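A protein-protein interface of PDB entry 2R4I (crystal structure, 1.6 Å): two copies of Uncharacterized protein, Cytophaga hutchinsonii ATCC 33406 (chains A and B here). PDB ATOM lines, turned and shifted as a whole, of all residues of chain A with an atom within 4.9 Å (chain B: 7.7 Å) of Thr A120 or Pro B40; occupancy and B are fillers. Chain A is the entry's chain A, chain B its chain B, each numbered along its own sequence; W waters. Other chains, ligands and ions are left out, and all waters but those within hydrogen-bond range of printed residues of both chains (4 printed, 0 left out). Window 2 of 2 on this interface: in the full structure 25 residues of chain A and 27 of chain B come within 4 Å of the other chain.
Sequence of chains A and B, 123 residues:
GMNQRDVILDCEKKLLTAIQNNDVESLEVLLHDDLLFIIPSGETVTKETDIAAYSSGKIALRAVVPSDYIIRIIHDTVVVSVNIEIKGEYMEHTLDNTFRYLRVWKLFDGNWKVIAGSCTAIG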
ATOM      1  N   PRO A  40     -27.039 -16.544  14.362  1.00  0.00           N
ATOM      2  CA  PRO A  40     -26.212 -17.715  13.988  1.00  0.00           C
ATOM      3  C   PRO A  40     -26.454 -19.082  14.642  1.00  0.00           C
ATOM      4  O   PRO A  40     -26.221 -20.130  14.003  1.00  0.00           O
ATOM      5  CB  PRO A  40     -24.784 -17.198  14.213  1.00  0.00           C
ATOM      6  CG  PRO A  40     -24.907 -15.736  13.935  1.00  0.00           C
ATOM      7  CD  PRO A  40     -26.205 -15.344  14.584  1.00  0.00           C
ATOM      8  N   THR A  98     -16.989 -10.170  11.219  1.00  0.00           N
ATOM      9  CA  THR A  98     -17.978  -9.702  10.237  1.00  0.00           C
ATOM     10  C   THR A  98     -19.098 -10.697  10.135  1.00  0.00           C
ATOM     11  O   THR A  98     -18.884 -11.923  10.243  1.00  0.00           O
ATOM     12  CB  THR A  98     -17.317  -9.479   8.830  1.00  0.00           C
ATOM     13  OG1 THR A  98     -16.445  -8.325   8.899  1.00  0.00           O
ATOM     14  CG2 THR A  98     -18.340  -9.277   7.736  1.00  0.00           C
ATOM     15  N   PHE A  99     -20.313 -10.173  10.002  1.00  0.00           N
ATOM     16  CA  PHE A  99     -21.492 -11.017   9.740  1.00  0.00           C
ATOM     17  C   PHE A  99     -22.158 -10.477   8.518  1.00  0.00           C
ATOM     18  O   PHE A  99     -22.130  -9.263   8.274  1.00  0.00           O
ATOM     19  CB  PHE A  99     -22.490 -11.026  10.903  1.00  0.00           C
ATOM     20  CG  PHE A  99     -21.877 -11.432  12.221  1.00  0.00           C
ATOM     21  CD1 PHE A  99     -21.094 -10.516  12.955  1.00  0.00           C
ATOM     22  CD2 PHE A  99     -22.078 -12.717  12.720  1.00  0.00           C
ATOM     23  CE1 PHE A  99     -20.500 -10.924  14.165  1.00  0.00           C
ATOM     24  CE2 PHE A  99     -21.487 -13.098  13.901  1.00  0.00           C
ATOM     25  CZ  PHE A  99     -20.705 -12.178  14.618  1.00  0.00           C
ATOM     26  N   ARG A 100     -22.808 -11.352   7.766  1.00  0.00           N
ATOM     27  CA  ARG A 100     -23.620 -10.932   6.619  1.00  0.00           C
ATOM     28  C   ARG A 100     -25.054 -10.757   7.125  1.00  0.00           C
ATOM     29  O   ARG A 100     -25.679 -11.736   7.511  1.00  0.00           O
ATOM     30  CB  ARG A 100     -23.563 -11.886   5.400  1.00  0.00           C
ATOM     31  CG  ARG A 100     -24.171 -11.237   4.155  1.00  0.00           C
ATOM     32  CD  ARG A 100     -23.128 -10.341   3.479  1.00  0.00           C
ATOM     33  NE  ARG A 100     -23.728  -9.490   2.447  1.00  0.00           N
ATOM     34  CZ  ARG A 100     -23.053  -8.823   1.517  1.00  0.00           C
ATOM     35  NH1 ARG A 100     -21.724  -8.881   1.505  1.00  0.00           N
ATOM     36  NH2 ARG A 100     -23.710  -8.100   0.592  1.00  0.00           N
ATOM     37  N   SER A 118     -31.806 -11.546   9.244  1.00  0.00           N
ATOM     38  CA  SER A 118     -30.957 -12.601   9.738  1.00  0.00           C
ATOM     39  C   SER A 118     -29.495 -12.162   9.762  1.00  0.00           C
ATOM     40  O   SER A 118     -29.110 -11.176   9.129  1.00  0.00           O
ATOM     41  CB  SER A 118     -31.119 -13.895   8.945  1.00  0.00           C
ATOM     42  OG  SER A 118     -30.705 -13.687   7.621  1.00  0.00           O
ATOM     43  N   CYS A 119     -28.727 -12.866  10.589  1.00  0.00           N
ATOM     44  CA  CYS A 119     -27.307 -12.596  10.824  1.00  0.00           C
ATOM     45  C   CYS A 119     -26.552 -13.885  10.540  1.00  0.00           C
ATOM     46  O   CYS A 119     -26.809 -14.905  11.187  1.00  0.00           O
ATOM     47  CB  CYS A 119     -27.109 -12.208  12.312  1.00  0.00           C
ATOM     48  SG  CYS A 119     -25.443 -11.969  12.757  1.00  0.00           S
ATOM     49  N   THR A 120     -25.659 -13.861   9.542  1.00  0.00           N
ATOM     50  CA  THR A 120     -24.892 -15.042   9.142  1.00  0.00           C
ATOM     51  C   THR A 120     -23.430 -14.851   9.511  1.00  0.00           C
ATOM     52  O   THR A 120     -22.800 -13.909   9.051  1.00  0.00           O
ATOM     53  CB  THR A 120     -25.008 -15.272   7.594  1.00  0.00           C
ATOM     54  OG1 THR A 120     -26.357 -15.632   7.251  1.00  0.00           O
ATOM     55  CG2 THR A 120     -24.061 -16.361   7.095  1.00  0.00           C
ATOM     56  N   ALA A 121     -22.877 -15.770  10.284  1.00  0.00           N
ATOM     57  CA  ALA A 121     -21.491 -15.689  10.687  1.00  0.00           C
ATOM     58  C   ALA A 121     -20.590 -16.238   9.583  1.00  0.00           C
ATOM     59  O   ALA A 121     -20.977 -17.121   8.849  1.00  0.00           O
ATOM     60  CB  ALA A 121     -21.281 -16.522  11.963  1.00  0.00           C
ATOM     61  N   ILE A 122     -19.412 -15.680   9.480  1.00  0.00           N
ATOM     62  CA  ILE A 122     -18.377 -16.139   8.539  1.00  0.00           C
ATOM     63  C   ILE A 122     -17.499 -17.119   9.333  1.00  0.00           C
ATOM     64  O   ILE A 122     -16.817 -16.727  10.301  1.00  0.00           O
ATOM     65  CB  ILE A 122     -17.589 -14.950   7.970  1.00  0.00           C
ATOM     66  CG1 ILE A 122     -18.520 -14.062   7.136  1.00  0.00           C
ATOM     67  CG2 ILE A 122     -16.388 -15.468   7.149  1.00  0.00           C
ATOM     68  CD1 ILE A 122     -17.894 -12.800   6.568  1.00  0.00           C
ATOM     69  N   ILE B  38     -29.602 -15.155   1.447  1.00  0.00           N
ATOM     70  CA  ILE B  38     -28.269 -15.334   2.077  1.00  0.00           C
ATOM     71  C   ILE B  38     -28.090 -16.839   2.320  1.00  0.00           C
ATOM     72  O   ILE B  38     -28.986 -17.489   2.831  1.00  0.00           O
ATOM     73  CB  ILE B  38     -28.077 -14.596   3.419  1.00  0.00           C
ATOM     74  CG1 ILE B  38     -28.429 -13.105   3.305  1.00  0.00           C
ATOM     75  CG2 ILE B  38     -26.661 -14.796   3.935  1.00  0.00           C
ATOM     76  CD1 ILE B  38     -27.672 -12.325   2.212  1.00  0.00           C
ATOM     77  N   ILE B  39     -26.931 -17.388   1.951  1.00  0.00           N
ATOM     78  CA  ILE B  39     -26.662 -18.834   2.143  1.00  0.00           C
ATOM     79  C   ILE B  39     -25.589 -18.987   3.222  1.00  0.00           C
ATOM     80  O   ILE B  39     -24.979 -18.008   3.615  1.00  0.00           O
ATOM     81  CB  ILE B  39     -26.325 -19.543   0.831  1.00  0.00           C
ATOM     82  CG1 ILE B  39     -25.115 -18.915   0.120  1.00  0.00           C
ATOM     83  CG2 ILE B  39     -27.545 -19.496  -0.073  1.00  0.00           C
ATOM     84  CD1 ILE B  39     -24.618 -19.717  -1.082  1.00  0.00           C
ATOM     85  N   PRO B  40     -25.370 -20.229   3.739  1.00  0.00           N
ATOM     86  CA  PRO B  40     -24.427 -20.392   4.858  1.00  0.00           C
ATOM     87  C   PRO B  40     -23.009 -19.830   4.738  1.00  0.00           C
ATOM     88  O   PRO B  40     -22.438 -19.426   5.752  1.00  0.00           O
ATOM     89  CB  PRO B  40     -24.433 -21.908   5.109  1.00  0.00           C
ATOM     90  CG  PRO B  40     -25.851 -22.335   4.680  1.00  0.00           C
ATOM     91  CD  PRO B  40     -26.099 -21.491   3.460  1.00  0.00           C
ATOM     92  N   SER B  41     -22.480 -19.730   3.511  1.00  0.00           N
ATOM     93  CA  SER B  41     -21.160 -19.158   3.272  1.00  0.00           C
ATOM     94  C   SER B  41     -21.139 -17.626   3.444  1.00  0.00           C
ATOM     95  O   SER B  41     -20.057 -17.028   3.434  1.00  0.00           O
ATOM     96  CB  SER B  41     -20.733 -19.452   1.831  1.00  0.00           C
ATOM     97  OG  SER B  41     -21.603 -18.845   0.910  1.00  0.00           O
ATOM     98  N   GLY B  42     -22.314 -17.010   3.589  1.00  0.00           N
ATOM     99  CA  GLY B  42     -22.421 -15.570   3.627  1.00  0.00           C
ATOM    100  C   GLY B  42     -22.667 -14.921   2.285  1.00  0.00           C
ATOM    101  O   GLY B  42     -22.909 -13.710   2.223  1.00  0.00           O
ATOM    102  N   GLU B  43     -22.693 -15.699   1.190  1.00  0.00           N
ATOM    103  CA  GLU B  43     -22.921 -15.145  -0.128  1.00  0.00           C
ATOM    104  C   GLU B  43     -24.376 -14.769  -0.319  1.00  0.00           C
ATOM    105  O   GLU B  43     -25.253 -15.341   0.325  1.00  0.00           O
ATOM    106  CB  GLU B  43     -22.464 -16.138  -1.203  1.00  0.00           C
ATOM    107  CG  GLU B  43     -20.964 -16.344  -1.126  1.00  0.00           C
ATOM    108  CD  GLU B  43     -20.456 -17.268  -2.197  1.00  0.00           C
ATOM    109  OE1 GLU B  43     -19.635 -16.833  -3.027  1.00  0.00           O
ATOM    110  OE2 GLU B  43     -20.938 -18.428  -2.187  1.00  0.00           O
ATOM    111  N   TYR B  90     -26.416 -31.613  -3.464  1.00  0.00           N
ATOM    112  CA  TYR B  90     -26.487 -30.160  -3.664  1.00  0.00           C
ATOM    113  C   TYR B  90     -25.152 -29.661  -4.202  1.00  0.00           C
ATOM    114  O   TYR B  90     -24.209 -29.471  -3.429  1.00  0.00           O
ATOM    115  CB  TYR B  90     -26.865 -29.430  -2.375  1.00  0.00           C
ATOM    116  CG  TYR B  90     -27.105 -27.962  -2.581  1.00  0.00           C
ATOM    117  CD1 TYR B  90     -26.086 -27.034  -2.425  1.00  0.00           C
ATOM    118  CD2 TYR B  90     -28.364 -27.507  -2.930  1.00  0.00           C
ATOM    119  CE1 TYR B  90     -26.323 -25.683  -2.622  1.00  0.00           C
ATOM    120  CE2 TYR B  90     -28.615 -26.169  -3.126  1.00  0.00           C
ATOM    121  CZ  TYR B  90     -27.593 -25.262  -2.974  1.00  0.00           C
ATOM    122  OH  TYR B  90     -27.862 -23.924  -3.159  1.00  0.00           O
ATOM    123  N   PHE B  99     -31.377 -27.071   8.890  1.00  0.00           N
ATOM    124  CA  PHE B  99     -31.227 -25.667   8.655  1.00  0.00           C
ATOM    125  C   PHE B  99     -32.369 -24.886   9.259  1.00  0.00           C
ATOM    126  O   PHE B  99     -33.488 -25.394   9.355  1.00  0.00           O
ATOM    127  CB  PHE B  99     -31.208 -25.367   7.160  1.00  0.00           C
ATOM    128  CG  PHE B  99     -30.135 -26.075   6.403  1.00  0.00           C
ATOM    129  CD1 PHE B  99     -30.418 -27.289   5.788  1.00  0.00           C
ATOM    130  CD2 PHE B  99     -28.859 -25.549   6.290  1.00  0.00           C
ATOM    131  CE1 PHE B  99     -29.431 -27.984   5.087  1.00  0.00           C
ATOM    132  CE2 PHE B  99     -27.844 -26.245   5.576  1.00  0.00           C
ATOM    133  CZ  PHE B  99     -28.134 -27.448   4.986  1.00  0.00           C
ATOM    134  N   ARG B 100     -32.100 -23.634   9.635  1.00  0.00           N
ATOM    135  CA  ARG B 100     -33.204 -22.700   9.967  1.00  0.00           C
ATOM    136  C   ARG B 100     -33.311 -21.703   8.806  1.00  0.00           C
ATOM    137  O   ARG B 100     -32.332 -20.970   8.501  1.00  0.00           O
ATOM    138  CB  ARG B 100     -33.022 -21.970  11.292  1.00  0.00           C
ATOM    139  CG  ARG B 100     -34.293 -21.363  11.792  1.00  0.00           C
ATOM    140  CD  ARG B 100     -35.147 -22.389  12.468  1.00  0.00           C
ATOM    141  NE  ARG B 100     -36.501 -21.847  12.672  1.00  0.00           N
ATOM    142  CZ  ARG B 100     -37.431 -22.417  13.423  1.00  0.00           C
ATOM    143  NH1 ARG B 100     -37.203 -23.551  14.006  1.00  0.00           N
ATOM    144  NH2 ARG B 100     -38.608 -21.840  13.553  1.00  0.00           N
ATOM    145  N   TYR B 101     -34.477 -21.700   8.173  1.00  0.00           N
ATOM    146  CA  TYR B 101     -34.760 -20.793   7.067  1.00  0.00           C
ATOM    147  C   TYR B 101     -35.617 -19.647   7.527  1.00  0.00           C
ATOM    148  O   TYR B 101     -36.558 -19.821   8.337  1.00  0.00           O
ATOM    149  CB  TYR B 101     -35.490 -21.500   5.901  1.00  0.00           C
ATOM    150  CG  TYR B 101     -34.595 -22.269   4.975  1.00  0.00           C
ATOM    151  CD1 TYR B 101     -34.114 -23.534   5.310  1.00  0.00           C
ATOM    152  CD2 TYR B 101     -34.258 -21.744   3.751  1.00  0.00           C
ATOM    153  CE1 TYR B 101     -33.288 -24.221   4.445  1.00  0.00           C
ATOM    154  CE2 TYR B 101     -33.460 -22.441   2.865  1.00  0.00           C
ATOM    155  CZ  TYR B 101     -32.978 -23.663   3.205  1.00  0.00           C
ATOM    156  OH  TYR B 101     -32.186 -24.321   2.293  1.00  0.00           O
ATOM    157  N   GLY B 117     -34.861 -14.073   1.893  1.00  0.00           N
ATOM    158  CA  GLY B 117     -34.685 -15.187   2.796  1.00  0.00           C
ATOM    159  C   GLY B 117     -33.266 -15.521   3.090  1.00  0.00           C
ATOM    160  O   GLY B 117     -32.336 -14.898   2.545  1.00  0.00           O
ATOM    161  N   SER B 118     -33.087 -16.511   3.954  1.00  0.00           N
ATOM    162  CA  SER B 118     -31.752 -16.985   4.304  1.00  0.00           C
ATOM    163  C   SER B 118     -31.826 -18.381   4.879  1.00  0.00           C
ATOM    164  O   SER B 118     -32.868 -18.805   5.339  1.00  0.00           O
ATOM    165  CB  SER B 118     -31.074 -16.029   5.295  1.00  0.00           C
ATOM    166  OG  SER B 118     -31.715 -15.995   6.556  1.00  0.00           O
ATOM    167  N   CYS B 119     -30.685 -19.058   4.817  1.00  0.00           N
ATOM    168  CA  CYS B 119     -30.493 -20.415   5.248  1.00  0.00           C
ATOM    169  C   CYS B 119     -29.359 -20.442   6.256  1.00  0.00           C
ATOM    170  O   CYS B 119     -28.254 -20.043   5.929  1.00  0.00           O
ATOM    171  CB  CYS B 119     -30.114 -21.258   4.004  1.00  0.00           C
ATOM    172  SG  CYS B 119     -29.578 -22.862   4.422  1.00  0.00           S
ATOM    173  N   THR B 120     -29.634 -20.907   7.475  1.00  0.00           N
ATOM    174  CA  THR B 120     -28.653 -20.987   8.546  1.00  0.00           C
ATOM    175  C   THR B 120     -28.442 -22.447   8.919  1.00  0.00           C
ATOM    176  O   THR B 120     -29.375 -23.119   9.281  1.00  0.00           O
ATOM    177  CB  THR B 120     -29.120 -20.191   9.800  1.00  0.00           C
ATOM    178  OG1 THR B 120     -29.228 -18.802   9.474  1.00  0.00           O
ATOM    179  CG2 THR B 120     -28.132 -20.377  10.978  1.00  0.00           C
ATOM    180  N   ALA B 121     -27.197 -22.909   8.872  1.00  0.00           N
ATOM    181  CA  ALA B 121     -26.896 -24.268   9.195  1.00  0.00           C
ATOM    182  C   ALA B 121     -26.993 -24.492  10.707  1.00  0.00           C
ATOM    183  O   ALA B 121     -26.491 -23.658  11.466  1.00  0.00           O
ATOM    184  CB  ALA B 121     -25.497 -24.650   8.672  1.00  0.00           C
ATOM    185  N   ILE B 122     -27.712 -25.545  11.121  1.00  0.00           N
ATOM    186  CA  ILE B 122     -27.836 -25.923  12.549  1.00  0.00           C
ATOM    187  C   ILE B 122     -27.064 -27.216  12.787  1.00  0.00           C
ATOM    188  O   ILE B 122     -27.355 -28.197  12.120  1.00  0.00           O
ATOM    189  CB  ILE B 122     -29.298 -26.146  12.981  1.00  0.00           C
ATOM    190  CG1 ILE B 122     -30.107 -24.874  12.861  1.00  0.00           C
ATOM    191  CG2 ILE B 122     -29.358 -26.670  14.430  1.00  0.00           C
ATOM    192  CD1 ILE B 122     -31.547 -25.151  13.146  1.00  0.00           C
HETATM  193  O   HOH W   1     -27.092 -17.366  10.666  1.00  0.00           O
HETATM  194  O   HOH W   2     -26.653 -18.494   7.367  1.00  0.00           O
HETATM  195  O   HOH W   3     -26.093 -22.736  14.106  1.00  0.00           O
HETATM  196  O   HOH W   4     -22.921 -11.690   0.356  1.00  0.00           O
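Printed residues of chain B within 4 Å of Thr A120: Ile B38 (3.4 Å), Ile B39 (3.96 Å), Pro B40 (3.7 Å) and Gly B42 (3.9 Å). Of the printed residues of chain A, Ile B38 touches Thr A120. Of the printed residues of chain A, Ile B39 touches Thr A120. Of chain A, only Thr A120 (3.7 Å) comes within 4 Å of Pro B40. Of the printed residues of chain A, Ser B118 touches Ser A118. The nearest printed residue of chain B that does not touch Thr A120 is Thr B120 (4.8 Å). The nearest residue of chain A that does not touch Pro B40 is Ala A121 (4.1 Å). The nearest printed residue of chain A that does not touch Ile B39 is Arg A100 (6.5 Å).
N of Arg A100 is in hydrogen-bond range of O of Thr A120 (2.9 Å). N of Arg B100 is in hydrogen-bond range of O of Thr B120 (2.8 Å). The backbone carbonyl oxygen of Ile B38 sits at hydrogen-bond distance from the backbone NH of Cys B119 (3.0 Å). O of Gly B117 is in hydrogen-bond range of N of Ile B38 (3.0 Å).
Among the printed residues, merely in contact across the chains: Arg A100 with Gly B42, Thr A120 with Ile B38, Pro A40 with Thr B120, Thr A120 with Pro B40, Thr A120 with Gly B42 and Thr A120 with Ile B39.
The side-chain hydroxyl (OG) of Ser A118 is in hydrogen-bond range of the side-chain hydroxyl (OG) of Ser B118, at 2.7 Å.
Pro A40 touches Thr B120, and with the chains exchanged Thr A120 touches Pro B40. Ser A118 touches its own counterpart, Ser B118. 8 positions are printed for both chains. Of the 7 pairs that touch across the chains among the printed residues, 3 have their exchanged pair printed and touching as well.
Water W1 bridges the backbone carbonyl oxygen of Cys A119 (2.5 Å) and the side-chain hydroxyl of Thr B120 (2.8 Å). Water W3 bridges the backbone carbonyl oxygen of Pro A40 (2.6 Å) and the backbone carbonyl oxygen of Ala B121 (2.8 Å). Water W2 lies within hydrogen-bond range of O of Cys B119 (2.7 Å), OG1 of Thr A120 (2.9 Å) and OG1 of Thr B120 (3.3 Å). Water W4 bridges O of Gly B42 (2.8 Å) and NE of Arg A100 (3.1 Å).
Of the 16 printed residues of chain B, 6 touch a printed residue of chain A. Hydrophobic or aromatic side chains of chain B that line the printed part of chain A: Ile B38.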
